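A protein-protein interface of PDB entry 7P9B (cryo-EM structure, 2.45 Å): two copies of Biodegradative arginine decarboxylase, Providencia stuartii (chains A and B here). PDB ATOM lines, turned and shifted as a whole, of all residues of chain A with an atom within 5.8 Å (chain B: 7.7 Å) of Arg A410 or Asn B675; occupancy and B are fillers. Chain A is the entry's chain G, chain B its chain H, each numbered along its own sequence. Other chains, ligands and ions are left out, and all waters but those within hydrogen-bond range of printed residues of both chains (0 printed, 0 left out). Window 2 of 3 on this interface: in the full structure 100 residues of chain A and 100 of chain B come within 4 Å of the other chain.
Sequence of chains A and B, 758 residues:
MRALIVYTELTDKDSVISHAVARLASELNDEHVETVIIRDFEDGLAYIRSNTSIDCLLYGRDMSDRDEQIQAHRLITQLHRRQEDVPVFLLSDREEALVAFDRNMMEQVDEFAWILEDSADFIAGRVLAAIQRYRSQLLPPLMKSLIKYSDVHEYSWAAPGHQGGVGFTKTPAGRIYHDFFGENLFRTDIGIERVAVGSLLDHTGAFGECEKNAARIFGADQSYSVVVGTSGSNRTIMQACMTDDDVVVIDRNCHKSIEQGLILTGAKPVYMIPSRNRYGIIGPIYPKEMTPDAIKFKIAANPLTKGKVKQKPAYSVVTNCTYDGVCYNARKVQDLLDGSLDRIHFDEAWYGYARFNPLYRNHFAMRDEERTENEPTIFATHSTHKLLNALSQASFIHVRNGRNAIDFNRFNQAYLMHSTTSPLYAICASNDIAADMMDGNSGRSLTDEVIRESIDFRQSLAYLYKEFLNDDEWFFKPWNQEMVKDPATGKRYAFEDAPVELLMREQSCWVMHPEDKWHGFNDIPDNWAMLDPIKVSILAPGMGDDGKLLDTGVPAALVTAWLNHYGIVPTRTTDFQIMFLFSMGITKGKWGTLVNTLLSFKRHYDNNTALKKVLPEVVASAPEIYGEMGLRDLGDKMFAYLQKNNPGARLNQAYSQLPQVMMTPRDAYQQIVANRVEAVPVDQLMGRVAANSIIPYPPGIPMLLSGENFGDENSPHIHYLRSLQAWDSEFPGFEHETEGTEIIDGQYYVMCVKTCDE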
ATOM      1  N   ALA A 240       2.572   6.249  21.079  1.00  0.00           N
ATOM      2  CA  ALA A 240       2.891   7.134  19.968  1.00  0.00           C
ATOM      3  C   ALA A 240       2.514   6.549  18.616  1.00  0.00           C
ATOM      4  O   ALA A 240       2.249   7.308  17.684  1.00  0.00           O
ATOM      5  CB  ALA A 240       4.376   7.468  19.971  1.00  0.00           C
ATOM      6  N   ARG A 343       6.040   0.555  10.578  1.00  0.00           N
ATOM      7  CA  ARG A 343       6.682   0.676  11.878  1.00  0.00           C
ATOM      8  C   ARG A 343       6.860  -0.711  12.465  1.00  0.00           C
ATOM      9  O   ARG A 343       5.894  -1.471  12.563  1.00  0.00           O
ATOM     10  CB  ARG A 343       5.859   1.537  12.833  1.00  0.00           C
ATOM     11  CG  ARG A 343       5.602   2.939  12.364  1.00  0.00           C
ATOM     12  CD  ARG A 343       4.962   3.685  13.485  1.00  0.00           C
ATOM     13  NE  ARG A 343       4.548   5.031  13.133  1.00  0.00           N
ATOM     14  CZ  ARG A 343       3.300   5.367  12.853  1.00  0.00           C
ATOM     15  NH1 ARG A 343       2.348   4.456  12.904  1.00  0.00           N
ATOM     16  NH2 ARG A 343       3.008   6.617  12.551  1.00  0.00           N
ATOM     17  N   ASN A 404       6.820   6.703   7.368  1.00  0.00           N
ATOM     18  CA  ASN A 404       5.776   7.071   8.319  1.00  0.00           C
ATOM     19  C   ASN A 404       6.362   7.314   9.708  1.00  0.00           C
ATOM     20  O   ASN A 404       5.828   6.870  10.724  1.00  0.00           O
ATOM     21  CB  ASN A 404       4.684   6.003   8.355  1.00  0.00           C
ATOM     22  CG  ASN A 404       3.427   6.481   9.023  1.00  0.00           C
ATOM     23  OD1 ASN A 404       3.336   7.632   9.444  1.00  0.00           O
ATOM     24  ND2 ASN A 404       2.446   5.599   9.139  1.00  0.00           N
ATOM     25  N   ALA A 405       7.483   8.024   9.742  1.00  0.00           N
ATOM     26  CA  ALA A 405       8.183   8.267  10.989  1.00  0.00           C
ATOM     27  C   ALA A 405       7.426   9.272  11.851  1.00  0.00           C
ATOM     28  O   ALA A 405       6.561  10.013  11.382  1.00  0.00           O
ATOM     29  CB  ALA A 405       9.597   8.768  10.717  1.00  0.00           C
ATOM     30  N   ILE A 406       7.768   9.286  13.133  1.00  0.00           N
ATOM     31  CA  ILE A 406       7.146  10.165  14.114  1.00  0.00           C
ATOM     32  C   ILE A 406       8.182  11.196  14.527  1.00  0.00           C
ATOM     33  O   ILE A 406       9.184  10.853  15.165  1.00  0.00           O
ATOM     34  CB  ILE A 406       6.641   9.377  15.329  1.00  0.00           C
ATOM     35  CG1 ILE A 406       5.698   8.265  14.883  1.00  0.00           C
ATOM     36  CG2 ILE A 406       5.926  10.299  16.287  1.00  0.00           C
ATOM     37  CD1 ILE A 406       5.427   7.248  15.942  1.00  0.00           C
ATOM     38  N   ASP A 407       7.947  12.454  14.174  1.00  0.00           N
ATOM     39  CA  ASP A 407       8.905  13.498  14.500  1.00  0.00           C
ATOM     40  C   ASP A 407       8.919  13.769  16.002  1.00  0.00           C
ATOM     41  O   ASP A 407       8.097  13.259  16.765  1.00  0.00           O
ATOM     42  CB  ASP A 407       8.595  14.775  13.723  1.00  0.00           C
ATOM     43  CG  ASP A 407       7.190  15.263  13.955  1.00  0.00           C
ATOM     44  OD1 ASP A 407       6.427  14.540  14.617  1.00  0.00           O
ATOM     45  OD2 ASP A 407       6.848  16.368  13.487  1.00  0.00           O
ATOM     46  N   PHE A 408       9.868  14.605  16.419  1.00  0.00           N
ATOM     47  CA  PHE A 408      10.135  14.778  17.842  1.00  0.00           C
ATOM     48  C   PHE A 408       8.952  15.388  18.577  1.00  0.00           C
ATOM     49  O   PHE A 408       8.653  14.997  19.710  1.00  0.00           O
ATOM     50  CB  PHE A 408      11.372  15.643  18.045  1.00  0.00           C
ATOM     51  CG  PHE A 408      11.706  15.868  19.481  1.00  0.00           C
ATOM     52  CD1 PHE A 408      12.338  14.886  20.214  1.00  0.00           C
ATOM     53  CD2 PHE A 408      11.362  17.050  20.108  1.00  0.00           C
ATOM     54  CE1 PHE A 408      12.636  15.086  21.539  1.00  0.00           C
ATOM     55  CE2 PHE A 408      11.654  17.251  21.431  1.00  0.00           C
ATOM     56  CZ  PHE A 408      12.293  16.268  22.148  1.00  0.00           C
ATOM     57  N   ASN A 409       8.278  16.363  17.970  1.00  0.00           N
ATOM     58  CA  ASN A 409       7.191  17.035  18.672  1.00  0.00           C
ATOM     59  C   ASN A 409       6.027  16.089  18.920  1.00  0.00           C
ATOM     60  O   ASN A 409       5.361  16.169  19.957  1.00  0.00           O
ATOM     61  CB  ASN A 409       6.729  18.257  17.886  1.00  0.00           C
ATOM     62  CG  ASN A 409       7.753  19.359  17.878  1.00  0.00           C
ATOM     63  OD1 ASN A 409       8.397  19.632  18.888  1.00  0.00           O
ATOM     64  ND2 ASN A 409       7.913  20.005  16.735  1.00  0.00           N
ATOM     65  N   ARG A 410       5.761  15.191  17.979  1.00  0.00           N
ATOM     66  CA  ARG A 410       4.693  14.225  18.172  1.00  0.00           C
ATOM     67  C   ARG A 410       5.111  13.123  19.136  1.00  0.00           C
ATOM     68  O   ARG A 410       4.289  12.625  19.911  1.00  0.00           O
ATOM     69  CB  ARG A 410       4.276  13.650  16.822  1.00  0.00           C
ATOM     70  CG  ARG A 410       3.553  14.648  15.947  1.00  0.00           C
ATOM     71  CD  ARG A 410       3.296  14.124  14.552  1.00  0.00           C
ATOM     72  NE  ARG A 410       2.493  12.908  14.536  1.00  0.00           N
ATOM     73  CZ  ARG A 410       2.915  11.747  14.055  1.00  0.00           C
ATOM     74  NH1 ARG A 410       4.117  11.655  13.528  1.00  0.00           N
ATOM     75  NH2 ARG A 410       2.128  10.686  14.079  1.00  0.00           N
ATOM     76  N   PHE A 411       6.383  12.733  19.112  1.00  0.00           N
ATOM     77  CA  PHE A 411       6.821  11.643  19.972  1.00  0.00           C
ATOM     78  C   PHE A 411       6.953  12.087  21.420  1.00  0.00           C
ATOM     79  O   PHE A 411       6.751  11.282  22.336  1.00  0.00           O
ATOM     80  CB  PHE A 411       8.149  11.081  19.475  1.00  0.00           C
ATOM     81  CG  PHE A 411       8.588   9.856  20.208  1.00  0.00           C
ATOM     82  CD1 PHE A 411       8.091   8.616  19.865  1.00  0.00           C
ATOM     83  CD2 PHE A 411       9.463   9.946  21.270  1.00  0.00           C
ATOM     84  CE1 PHE A 411       8.480   7.495  20.540  1.00  0.00           C
ATOM     85  CE2 PHE A 411       9.848   8.824  21.950  1.00  0.00           C
ATOM     86  CZ  PHE A 411       9.360   7.598  21.582  1.00  0.00           C
ATOM     87  N   ASN A 412       7.285  13.355  21.650  1.00  0.00           N
ATOM     88  CA  ASN A 412       7.529  13.810  23.011  1.00  0.00           C
ATOM     89  C   ASN A 412       6.249  13.841  23.832  1.00  0.00           C
ATOM     90  O   ASN A 412       6.305  13.746  25.056  1.00  0.00           O
ATOM     91  CB  ASN A 412       8.180  15.190  22.997  1.00  0.00           C
ATOM     92  CG  ASN A 412       8.989  15.460  24.246  1.00  0.00           C
ATOM     93  OD1 ASN A 412       9.739  16.427  24.315  1.00  0.00           O
ATOM     94  ND2 ASN A 412       8.864  14.586  25.229  1.00  0.00           N
ATOM     95  N   GLN A 413       5.092  13.962  23.189  1.00  0.00           N
ATOM     96  CA  GLN A 413       3.842  13.924  23.939  1.00  0.00           C
ATOM     97  C   GLN A 413       3.619  12.546  24.548  1.00  0.00           C
ATOM     98  O   GLN A 413       3.279  12.421  25.730  1.00  0.00           O
ATOM     99  CB  GLN A 413       2.682  14.319  23.033  1.00  0.00           C
ATOM    100  CG  GLN A 413       2.808  15.726  22.492  1.00  0.00           C
ATOM    101  CD  GLN A 413       2.761  16.765  23.580  1.00  0.00           C
ATOM    102  OE1 GLN A 413       1.970  16.670  24.512  1.00  0.00           O
ATOM    103  NE2 GLN A 413       3.631  17.753  23.484  1.00  0.00           N
ATOM    104  N   ALA A 414       3.834  11.496  23.756  1.00  0.00           N
ATOM    105  CA  ALA A 414       3.777  10.143  24.292  1.00  0.00           C
ATOM    106  C   ALA A 414       4.879   9.910  25.312  1.00  0.00           C
ATOM    107  O   ALA A 414       4.681   9.192  26.295  1.00  0.00           O
ATOM    108  CB  ALA A 414       3.874   9.126  23.161  1.00  0.00           C
ATOM    109  N   TYR B 669      -5.428  14.207  21.425  1.00  0.00           N
ATOM    110  CA  TYR B 669      -4.190  13.441  21.382  1.00  0.00           C
ATOM    111  C   TYR B 669      -4.208  12.423  20.249  1.00  0.00           C
ATOM    112  O   TYR B 669      -3.182  12.176  19.609  1.00  0.00           O
ATOM    113  CB  TYR B 669      -3.933  12.743  22.713  1.00  0.00           C
ATOM    114  CG  TYR B 669      -2.703  11.893  22.623  1.00  0.00           C
ATOM    115  CD1 TYR B 669      -1.449  12.470  22.604  1.00  0.00           C
ATOM    116  CD2 TYR B 669      -2.796  10.520  22.494  1.00  0.00           C
ATOM    117  CE1 TYR B 669      -0.328  11.709  22.485  1.00  0.00           C
ATOM    118  CE2 TYR B 669      -1.679   9.751  22.380  1.00  0.00           C
ATOM    119  CZ  TYR B 669      -0.445  10.353  22.373  1.00  0.00           C
ATOM    120  OH  TYR B 669       0.684   9.593  22.258  1.00  0.00           O
ATOM    121  N   GLN B 670      -5.361  11.822  19.982  1.00  0.00           N
ATOM    122  CA  GLN B 670      -5.431  10.864  18.893  1.00  0.00           C
ATOM    123  C   GLN B 670      -5.386  11.536  17.535  1.00  0.00           C
ATOM    124  O   GLN B 670      -5.051  10.881  16.547  1.00  0.00           O
ATOM    125  CB  GLN B 670      -6.676  10.011  19.033  1.00  0.00           C
ATOM    126  CG  GLN B 670      -6.534   8.991  20.124  1.00  0.00           C
ATOM    127  CD  GLN B 670      -7.754   8.142  20.261  1.00  0.00           C
ATOM    128  OE1 GLN B 670      -8.794   8.439  19.683  1.00  0.00           O
ATOM    129  NE2 GLN B 670      -7.625   7.044  20.986  1.00  0.00           N
ATOM    130  N   GLN B 671      -5.723  12.817  17.463  1.00  0.00           N
ATOM    131  CA  GLN B 671      -5.404  13.573  16.260  1.00  0.00           C
ATOM    132  C   GLN B 671      -3.902  13.737  16.117  1.00  0.00           C
ATOM    133  O   GLN B 671      -3.373  13.714  15.003  1.00  0.00           O
ATOM    134  CB  GLN B 671      -6.096  14.930  16.284  1.00  0.00           C
ATOM    135  CG  GLN B 671      -7.586  14.812  16.332  1.00  0.00           C
ATOM    136  CD  GLN B 671      -8.133  14.084  15.139  1.00  0.00           C
ATOM    137  OE1 GLN B 671      -7.689  14.291  14.016  1.00  0.00           O
ATOM    138  NE2 GLN B 671      -9.090  13.206  15.375  1.00  0.00           N
ATOM    139  N   ILE B 672      -3.199  13.914  17.235  1.00  0.00           N
ATOM    140  CA  ILE B 672      -1.736  13.921  17.176  1.00  0.00           C
ATOM    141  C   ILE B 672      -1.218  12.598  16.625  1.00  0.00           C
ATOM    142  O   ILE B 672      -0.337  12.573  15.760  1.00  0.00           O
ATOM    143  CB  ILE B 672      -1.118  14.220  18.554  1.00  0.00           C
ATOM    144  CG1 ILE B 672      -1.442  15.632  19.008  1.00  0.00           C
ATOM    145  CG2 ILE B 672       0.381  14.021  18.516  1.00  0.00           C
ATOM    146  CD1 ILE B 672      -1.031  15.891  20.420  1.00  0.00           C
ATOM    147  N   VAL B 673      -1.744  11.482  17.127  1.00  0.00           N
ATOM    148  CA  VAL B 673      -1.260  10.170  16.703  1.00  0.00           C
ATOM    149  C   VAL B 673      -1.562   9.934  15.230  1.00  0.00           C
ATOM    150  O   VAL B 673      -0.730   9.400  14.491  1.00  0.00           O
ATOM    151  CB  VAL B 673      -1.863   9.063  17.586  1.00  0.00           C
ATOM    152  CG1 VAL B 673      -1.503   7.704  17.047  1.00  0.00           C
ATOM    153  CG2 VAL B 673      -1.367   9.201  18.991  1.00  0.00           C
ATOM    154  N   ALA B 674      -2.745  10.330  14.779  1.00  0.00           N
ATOM    155  CA  ALA B 674      -3.132  10.193  13.382  1.00  0.00           C
ATOM    156  C   ALA B 674      -2.400  11.157  12.462  1.00  0.00           C
ATOM    157  O   ALA B 674      -2.721  11.211  11.274  1.00  0.00           O
ATOM    158  CB  ALA B 674      -4.641  10.389  13.237  1.00  0.00           C
ATOM    159  N   ASN B 675      -1.438  11.913  12.984  1.00  0.00           N
ATOM    160  CA  ASN B 675      -0.654  12.887  12.230  1.00  0.00           C
ATOM    161  C   ASN B 675      -1.524  13.990  11.638  1.00  0.00           C
ATOM    162  O   ASN B 675      -1.152  14.618  10.648  1.00  0.00           O
ATOM    163  CB  ASN B 675       0.166  12.209  11.127  1.00  0.00           C
ATOM    164  CG  ASN B 675       1.294  13.079  10.622  1.00  0.00           C
ATOM    165  OD1 ASN B 675       1.500  14.189  11.105  1.00  0.00           O
ATOM    166  ND2 ASN B 675       2.027  12.583   9.639  1.00  0.00           N
ATOM    167  N   ARG B 676      -2.694  14.235  12.211  1.00  0.00           N
ATOM    168  CA  ARG B 676      -3.561  15.314  11.743  1.00  0.00           C
ATOM    169  C   ARG B 676      -3.323  16.595  12.531  1.00  0.00           C
ATOM    170  O   ARG B 676      -4.265  17.228  12.993  1.00  0.00           O
ATOM    171  CB  ARG B 676      -5.018  14.891  11.835  1.00  0.00           C
ATOM    172  CG  ARG B 676      -5.412  13.721  10.962  1.00  0.00           C
ATOM    173  CD  ARG B 676      -6.916  13.515  11.023  1.00  0.00           C
ATOM    174  NE  ARG B 676      -7.378  12.368  10.250  1.00  0.00           N
ATOM    175  CZ  ARG B 676      -7.637  11.171  10.766  1.00  0.00           C
ATOM    176  NH1 ARG B 676      -7.497  10.960  12.066  1.00  0.00           N
ATOM    177  NH2 ARG B 676      -8.055  10.184   9.986  1.00  0.00           N
ATOM    178  N   VAL B 677      -2.067  17.010  12.684  1.00  0.00           N
ATOM    179  CA  VAL B 677      -1.725  18.189  13.467  1.00  0.00           C
ATOM    180  C   VAL B 677      -0.615  18.954  12.762  1.00  0.00           C
ATOM    181  O   VAL B 677       0.055  18.440  11.866  1.00  0.00           O
ATOM    182  CB  VAL B 677      -1.290  17.853  14.913  1.00  0.00           C
ATOM    183  CG1 VAL B 677      -2.432  17.238  15.689  1.00  0.00           C
ATOM    184  CG2 VAL B 677      -0.084  16.934  14.903  1.00  0.00           C
ATOM    185  N   GLU B 678      -0.418  20.193  13.197  1.00  0.00           N
ATOM    186  CA  GLU B 678       0.535  21.087  12.560  1.00  0.00           C
ATOM    187  C   GLU B 678       0.864  22.239  13.494  1.00  0.00           C
ATOM    188  O   GLU B 678       0.021  22.692  14.266  1.00  0.00           O
ATOM    189  CB  GLU B 678      -0.015  21.615  11.233  1.00  0.00           C
ATOM    190  CG  GLU B 678      -1.309  22.382  11.382  1.00  0.00           C
ATOM    191  CD  GLU B 678      -1.878  22.837  10.058  1.00  0.00           C
ATOM    192  OE1 GLU B 678      -1.238  22.590   9.013  1.00  0.00           O
ATOM    193  OE2 GLU B 678      -2.977  23.429  10.056  1.00  0.00           O
ATOM    194  N   GLU B 742       6.329  25.594  21.068  1.00  0.00           N
ATOM    195  CA  GLU B 742       7.693  25.617  20.564  1.00  0.00           C
ATOM    196  C   GLU B 742       8.076  27.073  20.371  1.00  0.00           C
ATOM    197  O   GLU B 742       7.207  27.913  20.137  1.00  0.00           O
ATOM    198  CB  GLU B 742       7.815  24.857  19.244  1.00  0.00           C
ATOM    199  CG  GLU B 742       7.526  23.369  19.340  1.00  0.00           C
ATOM    200  CD  GLU B 742       6.050  23.039  19.181  1.00  0.00           C
ATOM    201  OE1 GLU B 742       5.256  23.959  18.910  1.00  0.00           O
ATOM    202  OE2 GLU B 742       5.683  21.855  19.323  1.00  0.00           O
ATOM    203  N   MET B 751       1.105  23.530  18.499  1.00  0.00           N
ATOM    204  CA  MET B 751       0.688  22.398  17.687  1.00  0.00           C
ATOM    205  C   MET B 751      -0.826  22.246  17.760  1.00  0.00           C
ATOM    206  O   MET B 751      -1.369  21.859  18.797  1.00  0.00           O
ATOM    207  CB  MET B 751       1.405  21.136  18.154  1.00  0.00           C
ATOM    208  CG  MET B 751       1.059  19.869  17.399  1.00  0.00           C
ATOM    209  SD  MET B 751       2.178  18.525  17.852  1.00  0.00           S
ATOM    210  CE  MET B 751       1.741  18.269  19.562  1.00  0.00           C
ATOM    211  N   LYS B 754      -5.239  19.884  12.529  1.00  0.00           N
ATOM    212  CA  LYS B 754      -5.496  20.306  11.158  1.00  0.00           C
ATOM    213  C   LYS B 754      -6.992  20.423  10.906  1.00  0.00           C
ATOM    214  O   LYS B 754      -7.784  19.619  11.401  1.00  0.00           O
ATOM    215  CB  LYS B 754      -4.887  19.322  10.162  1.00  0.00           C
ATOM    216  CG  LYS B 754      -3.381  19.358  10.049  1.00  0.00           C
ATOM    217  CD  LYS B 754      -2.938  18.360   9.000  1.00  0.00           C
ATOM    218  CE  LYS B 754      -1.455  18.104   9.057  1.00  0.00           C
ATOM    219  NZ  LYS B 754      -1.072  17.045   8.088  1.00  0.00           N
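The guanidinium group (NH2) of Arg A410 is in hydrogen-bond range of the backbone carbonyl oxygen (O) of Val B673, at 3.2 Å. O of Ile B672 lies within hydrogen-bond range of NE of Arg A410 (3.1 Å).
Of the 13 printed residues of chain B, 5 touch a printed residue of chain A. Along chain A the printed residues that touch a printed residue of chain B span positions 240 to 414. Among the printed residues, 6 pairs touch across the chains. Among the printed residues, no Asp or Glu carboxylate lies within 4 Å of a Lys or Arg side-chain nitrogen of the other chain.
The side-chain carboxylate of Asp A407 is in salt-bridge range of the guanidinium group of Arg A410, at 3.9 Å.
CG1 of Val B673 touches O of Ala A240 (3.8 Å). OE2 of Glu B742 touches OD1 of Asn A409, 3.5 Å away. OD1 of Asn B675 touches NE of Arg A410, at 3.8 Å. Tyr B669 touches Ala A414.
No position is printed for both chains. Of the 6 pairs that touch across the chains among the printed residues, none has its exchanged pair printed and touching as well.
Of the printed residues of chain B, Asn A409 touches Glu B742. Of chain B, only Ile B672 (3.1 Å), Val B673 (3.2 Å) and Asn B675 (3.8 Å) come within 4 Å of Arg A410. Phe A411 touches none of the printed residues of chain B. Of the printed residues of chain B, Ala A414 touches Tyr B669. Of the printed residues of chain A, Tyr B669 touches Ala A414. Of the printed residues of chain A, Ile B672 touches Arg A410 (3.1 Å). Printed residues of chain A within 4 Å of Val B673: Ala A240 (3.8 Å) and Arg A410 (3.2 Å). Asn B675 touches just one residue of chain A: Arg A410. The nearest residue of chain A that does not touch Asn B675 is Asn A404 (5.1 Å). The nearest printed residue of chain A that does not touch Glu B742 is Gln A413 (6.2 Å).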
